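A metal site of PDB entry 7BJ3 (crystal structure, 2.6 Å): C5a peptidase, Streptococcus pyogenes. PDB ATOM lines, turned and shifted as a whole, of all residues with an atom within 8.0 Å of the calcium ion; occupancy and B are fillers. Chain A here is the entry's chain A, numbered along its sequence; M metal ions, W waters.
Of the 23 residues printed, 5 come within 4 Å of the calcium ion.
The side-chain carboxylate of Asp 800 sits at hydrogen-bond distance from the backbone NH of Gly 797, at 2.7 Å.
N of Gly 795 lies close to OD2 of Asp 800, at 3.3 Å.
The side-chain amide nitrogen (ND2) of Asn 794 lies within hydrogen-bond range of the side-chain amide oxygen (OD1) of Asn 988 (3.5 Å).
ND2 of Asn 798 lies within hydrogen-bond range of O of Gly 987 (2.6 Å).
OE2 of Glu 983 lies within hydrogen-bond range of ND2 of Asn 798 (2.9 Å).
O of Asp 796 sits at hydrogen-bond distance from ND2 of Asn 736 (2.8 Å).
The backbone NH of Ser 792 is in hydrogen-bond range of the backbone carbonyl oxygen of Arg 799, 2.8 Å away.
The backbone NH (N) of Ser 792 lies within hydrogen-bond range of the backbone carbonyl oxygen (O) of Ala 986 (3.1 Å).
The calcium ion is bound by the side-chain carboxylate (OD1) of Asp 800, the side-chain amide oxygen (OD1) of Asn 794, the backbone carbonyl oxygen (O) of Asn 798, the side-chain carboxylate (OD1) of Asp 796, water W1, the backbone carbonyl oxygen (O) of Ser 792 and the side-chain hydroxyl (OG) of Ser 792.
The calcium ion has seven donor atoms within binding distance.
Water W1 lies within hydrogen-bond range of the side-chain carboxylate of Asp 796 (2.7 Å), the backbone carbonyl oxygen of Gly 987 (2.7 Å) and the side-chain amide nitrogen of Asn 794 (3.2 Å).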
ATOM      1  N   GLU A 734     -21.097  13.576   4.548  1.00  0.00           N
ATOM      2  CA  GLU A 734     -20.297  13.920   5.710  1.00  0.00           C
ATOM      3  C   GLU A 734     -20.323  12.768   6.717  1.00  0.00           C
ATOM      4  O   GLU A 734     -21.330  12.073   6.861  1.00  0.00           O
ATOM      5  CB  GLU A 734     -20.799  15.205   6.374  1.00  0.00           C
ATOM      6  CG  GLU A 734     -20.277  16.465   5.717  1.00  0.00           C
ATOM      7  CD  GLU A 734     -20.605  17.708   6.516  1.00  0.00           C
ATOM      8  OE1 GLU A 734     -21.806  17.975   6.715  1.00  0.00           O
ATOM      9  OE2 GLU A 734     -19.672  18.396   6.955  1.00  0.00           O
ATOM     10  N   ASN A 736     -19.879  12.167  10.720  1.00  0.00           N
ATOM     11  CA  ASN A 736     -19.919  12.879  11.992  1.00  0.00           C
ATOM     12  C   ASN A 736     -19.733  11.876  13.130  1.00  0.00           C
ATOM     13  O   ASN A 736     -20.637  11.061  13.374  1.00  0.00           O
ATOM     14  CB  ASN A 736     -21.243  13.629  12.150  1.00  0.00           C
ATOM     15  CG  ASN A 736     -21.142  14.778  13.117  1.00  0.00           C
ATOM     16  OD1 ASN A 736     -20.051  15.220  13.472  1.00  0.00           O
ATOM     17  ND2 ASN A 736     -22.294  15.280  13.559  1.00  0.00           N
ATOM     18  N   ILE A 741     -21.579  14.197  17.720  1.00  0.00           N
ATOM     19  CA  ILE A 741     -23.036  14.115  17.799  1.00  0.00           C
ATOM     20  C   ILE A 741     -23.491  14.298  19.237  1.00  0.00           C
ATOM     21  O   ILE A 741     -24.459  15.027  19.509  1.00  0.00           O
ATOM     22  CB  ILE A 741     -23.529  12.768  17.212  1.00  0.00           C
ATOM     23  CG1 ILE A 741     -23.155  12.657  15.742  1.00  0.00           C
ATOM     24  CG2 ILE A 741     -25.022  12.632  17.403  1.00  0.00           C
ATOM     25  CD1 ILE A 741     -23.521  11.334  15.113  1.00  0.00           C
ATOM     26  N   ALA A 790     -25.785   5.383   0.994  1.00  0.00           N
ATOM     27  CA  ALA A 790     -26.926   5.350   1.882  1.00  0.00           C
ATOM     28  C   ALA A 790     -26.873   6.541   2.828  1.00  0.00           C
ATOM     29  O   ALA A 790     -25.814   6.917   3.312  1.00  0.00           O
ATOM     30  CB  ALA A 790     -26.972   4.040   2.687  1.00  0.00           C
ATOM     31  N   ILE A 791     -28.042   7.141   3.066  1.00  0.00           N
ATOM     32  CA  ILE A 791     -28.171   8.268   3.988  1.00  0.00           C
ATOM     33  C   ILE A 791     -29.168   7.906   5.075  1.00  0.00           C
ATOM     34  O   ILE A 791     -30.045   7.055   4.909  1.00  0.00           O
ATOM     35  CB  ILE A 791     -28.601   9.560   3.275  1.00  0.00           C
ATOM     36  CG1 ILE A 791     -29.932   9.357   2.550  1.00  0.00           C
ATOM     37  CG2 ILE A 791     -27.521  10.042   2.316  1.00  0.00           C
ATOM     38  CD1 ILE A 791     -30.474  10.621   1.920  1.00  0.00           C
ATOM     39  N   SER A 792     -29.031   8.574   6.212  1.00  0.00           N
ATOM     40  CA  SER A 792     -29.948   8.442   7.348  1.00  0.00           C
ATOM     41  C   SER A 792     -30.403   9.841   7.737  1.00  0.00           C
ATOM     42  O   SER A 792     -29.864  10.449   8.674  1.00  0.00           O
ATOM     43  CB  SER A 792     -29.280   7.734   8.520  1.00  0.00           C
ATOM     44  OG  SER A 792     -28.015   8.299   8.801  1.00  0.00           O
ATOM     45  N   PRO A 793     -31.406  10.388   7.039  1.00  0.00           N
ATOM     46  CA  PRO A 793     -31.799  11.788   7.259  1.00  0.00           C
ATOM     47  C   PRO A 793     -32.447  12.017   8.617  1.00  0.00           C
ATOM     48  O   PRO A 793     -33.673  11.986   8.747  1.00  0.00           O
ATOM     49  CB  PRO A 793     -32.770  12.071   6.112  1.00  0.00           C
ATOM     50  CG  PRO A 793     -33.344  10.730   5.771  1.00  0.00           C
ATOM     51  CD  PRO A 793     -32.234   9.735   6.002  1.00  0.00           C
ATOM     52  N   ASN A 794     -31.629  12.254   9.646  1.00  0.00           N
ATOM     53  CA  ASN A 794     -32.133  12.496  10.994  1.00  0.00           C
ATOM     54  C   ASN A 794     -31.423  13.672  11.669  1.00  0.00           C
ATOM     55  O   ASN A 794     -31.426  13.771  12.896  1.00  0.00           O
ATOM     56  CB  ASN A 794     -32.002  11.234  11.856  1.00  0.00           C
ATOM     57  CG  ASN A 794     -30.651  10.564  11.724  1.00  0.00           C
ATOM     58  OD1 ASN A 794     -29.663  11.212  11.370  1.00  0.00           O
ATOM     59  ND2 ASN A 794     -30.604   9.273  11.988  1.00  0.00           N
ATOM     60  N   GLY A 795     -30.808  14.560  10.876  1.00  0.00           N
ATOM     61  CA  GLY A 795     -30.292  15.823  11.364  1.00  0.00           C
ATOM     62  C   GLY A 795     -29.085  15.756  12.272  1.00  0.00           C
ATOM     63  O   GLY A 795     -28.650  16.803  12.772  1.00  0.00           O
ATOM     64  N   ASP A 796     -28.506  14.574  12.490  1.00  0.00           N
ATOM     65  CA  ASP A 796     -27.344  14.449  13.379  1.00  0.00           C
ATOM     66  C   ASP A 796     -26.020  14.716  12.670  1.00  0.00           C
ATOM     67  O   ASP A 796     -24.975  14.634  13.315  1.00  0.00           O
ATOM     68  CB  ASP A 796     -27.320  13.058  14.020  1.00  0.00           C
ATOM     69  CG  ASP A 796     -26.978  11.950  13.035  1.00  0.00           C
ATOM     70  OD1 ASP A 796     -27.079  12.168  11.812  1.00  0.00           O
ATOM     71  OD2 ASP A 796     -26.611  10.844  13.495  1.00  0.00           O
ATOM     72  N   GLY A 797     -26.043  15.032  11.375  1.00  0.00           N
ATOM     73  CA  GLY A 797     -24.838  15.330  10.653  1.00  0.00           C
ATOM     74  C   GLY A 797     -24.057  14.131  10.156  1.00  0.00           C
ATOM     75  O   GLY A 797     -23.052  14.310   9.454  1.00  0.00           O
ATOM     76  N   ASN A 798     -24.482  12.922  10.489  1.00  0.00           N
ATOM     77  CA  ASN A 798     -23.792  11.699  10.087  1.00  0.00           C
ATOM     78  C   ASN A 798     -24.518  11.114   8.882  1.00  0.00           C
ATOM     79  O   ASN A 798     -25.550  10.457   9.022  1.00  0.00           O
ATOM     80  CB  ASN A 798     -23.745  10.698  11.238  1.00  0.00           C
ATOM     81  CG  ASN A 798     -22.940   9.462  10.897  1.00  0.00           C
ATOM     82  OD1 ASN A 798     -21.866   9.556  10.292  1.00  0.00           O
ATOM     83  ND2 ASN A 798     -23.450   8.294  11.286  1.00  0.00           N
ATOM     84  N   ARG A 799     -23.964  11.356   7.695  1.00  0.00           N
ATOM     85  CA  ARG A 799     -24.486  10.790   6.450  1.00  0.00           C
ATOM     86  C   ARG A 799     -25.961  11.146   6.247  1.00  0.00           C
ATOM     87  O   ARG A 799     -26.805  10.282   6.022  1.00  0.00           O
ATOM     88  CB  ARG A 799     -24.266   9.282   6.401  1.00  0.00           C
ATOM     89  CG  ARG A 799     -22.798   8.891   6.482  1.00  0.00           C
ATOM     90  CD  ARG A 799     -22.600   7.395   6.634  1.00  0.00           C
ATOM     91  NE  ARG A 799     -21.191   7.064   6.801  1.00  0.00           N
ATOM     92  CZ  ARG A 799     -20.418   6.593   5.822  1.00  0.00           C
ATOM     93  NH1 ARG A 799     -20.919   6.387   4.608  1.00  0.00           N
ATOM     94  NH2 ARG A 799     -19.143   6.326   6.070  1.00  0.00           N
ATOM     95  N   ASP A 800     -26.252  12.445   6.331  1.00  0.00           N
ATOM     96  CA  ASP A 800     -27.606  12.954   6.207  1.00  0.00           C
ATOM     97  C   ASP A 800     -27.978  13.323   4.767  1.00  0.00           C
ATOM     98  O   ASP A 800     -29.177  13.492   4.496  1.00  0.00           O
ATOM     99  CB  ASP A 800     -27.797  14.190   7.101  1.00  0.00           C
ATOM    100  CG  ASP A 800     -27.712  13.858   8.580  1.00  0.00           C
ATOM    101  OD1 ASP A 800     -27.528  12.673   8.919  1.00  0.00           O
ATOM    102  OD2 ASP A 800     -27.820  14.793   9.411  1.00  0.00           O
ATOM    103  N   TYR A 801     -27.009  13.445   3.869  1.00  0.00           N
ATOM    104  CA  TYR A 801     -27.288  13.959   2.533  1.00  0.00           C
ATOM    105  C   TYR A 801     -26.294  13.371   1.529  1.00  0.00           C
ATOM    106  O   TYR A 801     -25.274  12.797   1.891  1.00  0.00           O
ATOM    107  CB  TYR A 801     -27.212  15.487   2.508  1.00  0.00           C
ATOM    108  CG  TYR A 801     -25.816  16.053   2.691  1.00  0.00           C
ATOM    109  CD1 TYR A 801     -24.964  16.227   1.602  1.00  0.00           C
ATOM    110  CD2 TYR A 801     -25.356  16.411   3.948  1.00  0.00           C
ATOM    111  CE1 TYR A 801     -23.689  16.741   1.763  1.00  0.00           C
ATOM    112  CE2 TYR A 801     -24.079  16.922   4.123  1.00  0.00           C
ATOM    113  CZ  TYR A 801     -23.258  17.088   3.022  1.00  0.00           C
ATOM    114  OH  TYR A 801     -21.992  17.599   3.184  1.00  0.00           O
ATOM    115  N   ASP A 898     -32.638   5.302   4.952  1.00  0.00           N
ATOM    116  CA  ASP A 898     -33.021   4.458   6.085  1.00  0.00           C
ATOM    117  C   ASP A 898     -32.825   5.257   7.363  1.00  0.00           C
ATOM    118  O   ASP A 898     -31.702   5.609   7.717  1.00  0.00           O
ATOM    119  CB  ASP A 898     -32.187   3.182   6.103  1.00  0.00           C
ATOM    120  CG  ASP A 898     -32.839   2.077   6.917  1.00  0.00           C
ATOM    121  OD1 ASP A 898     -33.506   2.378   7.921  1.00  0.00           O
ATOM    122  OD2 ASP A 898     -32.675   0.898   6.540  1.00  0.00           O
ATOM    123  N   ASN A 899     -33.924   5.518   8.077  1.00  0.00           N
ATOM    124  CA  ASN A 899     -33.897   6.249   9.336  1.00  0.00           C
ATOM    125  C   ASN A 899     -33.934   5.348  10.555  1.00  0.00           C
ATOM    126  O   ASN A 899     -33.963   5.854  11.683  1.00  0.00           O
ATOM    127  CB  ASN A 899     -35.060   7.245   9.404  1.00  0.00           C
ATOM    128  CG  ASN A 899     -34.722   8.582   8.803  1.00  0.00           C
ATOM    129  OD1 ASN A 899     -33.581   9.038   8.884  1.00  0.00           O
ATOM    130  ND2 ASN A 899     -35.710   9.223   8.180  1.00  0.00           N
ATOM    131  N   GLU A 983     -23.180   1.410  14.695  1.00  0.00           N
ATOM    132  CA  GLU A 983     -23.521   2.220  13.534  1.00  0.00           C
ATOM    133  C   GLU A 983     -23.798   1.310  12.348  1.00  0.00           C
ATOM    134  O   GLU A 983     -23.086   0.325  12.135  1.00  0.00           O
ATOM    135  CB  GLU A 983     -22.369   3.186  13.212  1.00  0.00           C
ATOM    136  CG  GLU A 983     -22.659   4.195  12.126  1.00  0.00           C
ATOM    137  CD  GLU A 983     -21.442   5.042  11.815  1.00  0.00           C
ATOM    138  OE1 GLU A 983     -20.333   4.687  12.281  1.00  0.00           O
ATOM    139  OE2 GLU A 983     -21.581   6.058  11.103  1.00  0.00           O
ATOM    140  N   ASP A 984     -24.847   1.618  11.588  1.00  0.00           N
ATOM    141  CA  ASP A 984     -25.159   0.861  10.386  1.00  0.00           C
ATOM    142  C   ASP A 984     -24.678   1.620   9.143  1.00  0.00           C
ATOM    143  O   ASP A 984     -24.233   2.762   9.209  1.00  0.00           O
ATOM    144  CB  ASP A 984     -26.660   0.544  10.295  1.00  0.00           C
ATOM    145  CG  ASP A 984     -27.545   1.785  10.124  1.00  0.00           C
ATOM    146  OD1 ASP A 984     -27.036   2.885   9.824  1.00  0.00           O
ATOM    147  OD2 ASP A 984     -28.773   1.647  10.284  1.00  0.00           O
ATOM    148  N   ALA A 986     -26.121   3.042   6.816  1.00  0.00           N
ATOM    149  CA  ALA A 986     -26.830   4.256   6.441  1.00  0.00           C
ATOM    150  C   ALA A 986     -26.433   5.450   7.295  1.00  0.00           C
ATOM    151  O   ALA A 986     -26.743   6.592   6.929  1.00  0.00           O
ATOM    152  CB  ALA A 986     -28.340   4.031   6.529  1.00  0.00           C
ATOM    153  N   GLY A 987     -25.751   5.226   8.420  1.00  0.00           N
ATOM    154  CA  GLY A 987     -25.376   6.283   9.331  1.00  0.00           C
ATOM    155  C   GLY A 987     -26.101   6.247  10.662  1.00  0.00           C
ATOM    156  O   GLY A 987     -25.676   6.933  11.595  1.00  0.00           O
ATOM    157  N   ASN A 988     -27.178   5.474  10.772  1.00  0.00           N
ATOM    158  CA  ASN A 988     -27.887   5.352  12.040  1.00  0.00           C
ATOM    159  C   ASN A 988     -26.946   4.809  13.104  1.00  0.00           C
ATOM    160  O   ASN A 988     -26.292   3.785  12.906  1.00  0.00           O
ATOM    161  CB  ASN A 988     -29.109   4.456  11.884  1.00  0.00           C
ATOM    162  CG  ASN A 988     -30.105   4.983  10.869  1.00  0.00           C
ATOM    163  OD1 ASN A 988     -30.860   5.921  11.151  1.00  0.00           O
ATOM    164  ND2 ASN A 988     -30.112   4.387   9.684  1.00  0.00           N
ATOM    165  N   ILE A 989     -26.883   5.506  14.235  1.00  0.00           N
ATOM    166  CA  ILE A 989     -25.868   5.249  15.242  1.00  0.00           C
ATOM    167  C   ILE A 989     -26.490   5.351  16.622  1.00  0.00           C
ATOM    168  O   ILE A 989     -27.410   6.146  16.849  1.00  0.00           O
ATOM    169  CB  ILE A 989     -24.690   6.236  15.087  1.00  0.00           C
ATOM    170  CG1 ILE A 989     -23.556   5.907  16.049  1.00  0.00           C
ATOM    171  CG2 ILE A 989     -25.165   7.678  15.269  1.00  0.00           C
ATOM    172  CD1 ILE A 989     -22.332   6.794  15.869  1.00  0.00           C
HETATM  173 CA    CA M   1     -27.762  10.639  10.009  1.00  0.00          CA
HETATM  174  O   HOH W   1     -27.476   8.952  11.792  1.00  0.00           O
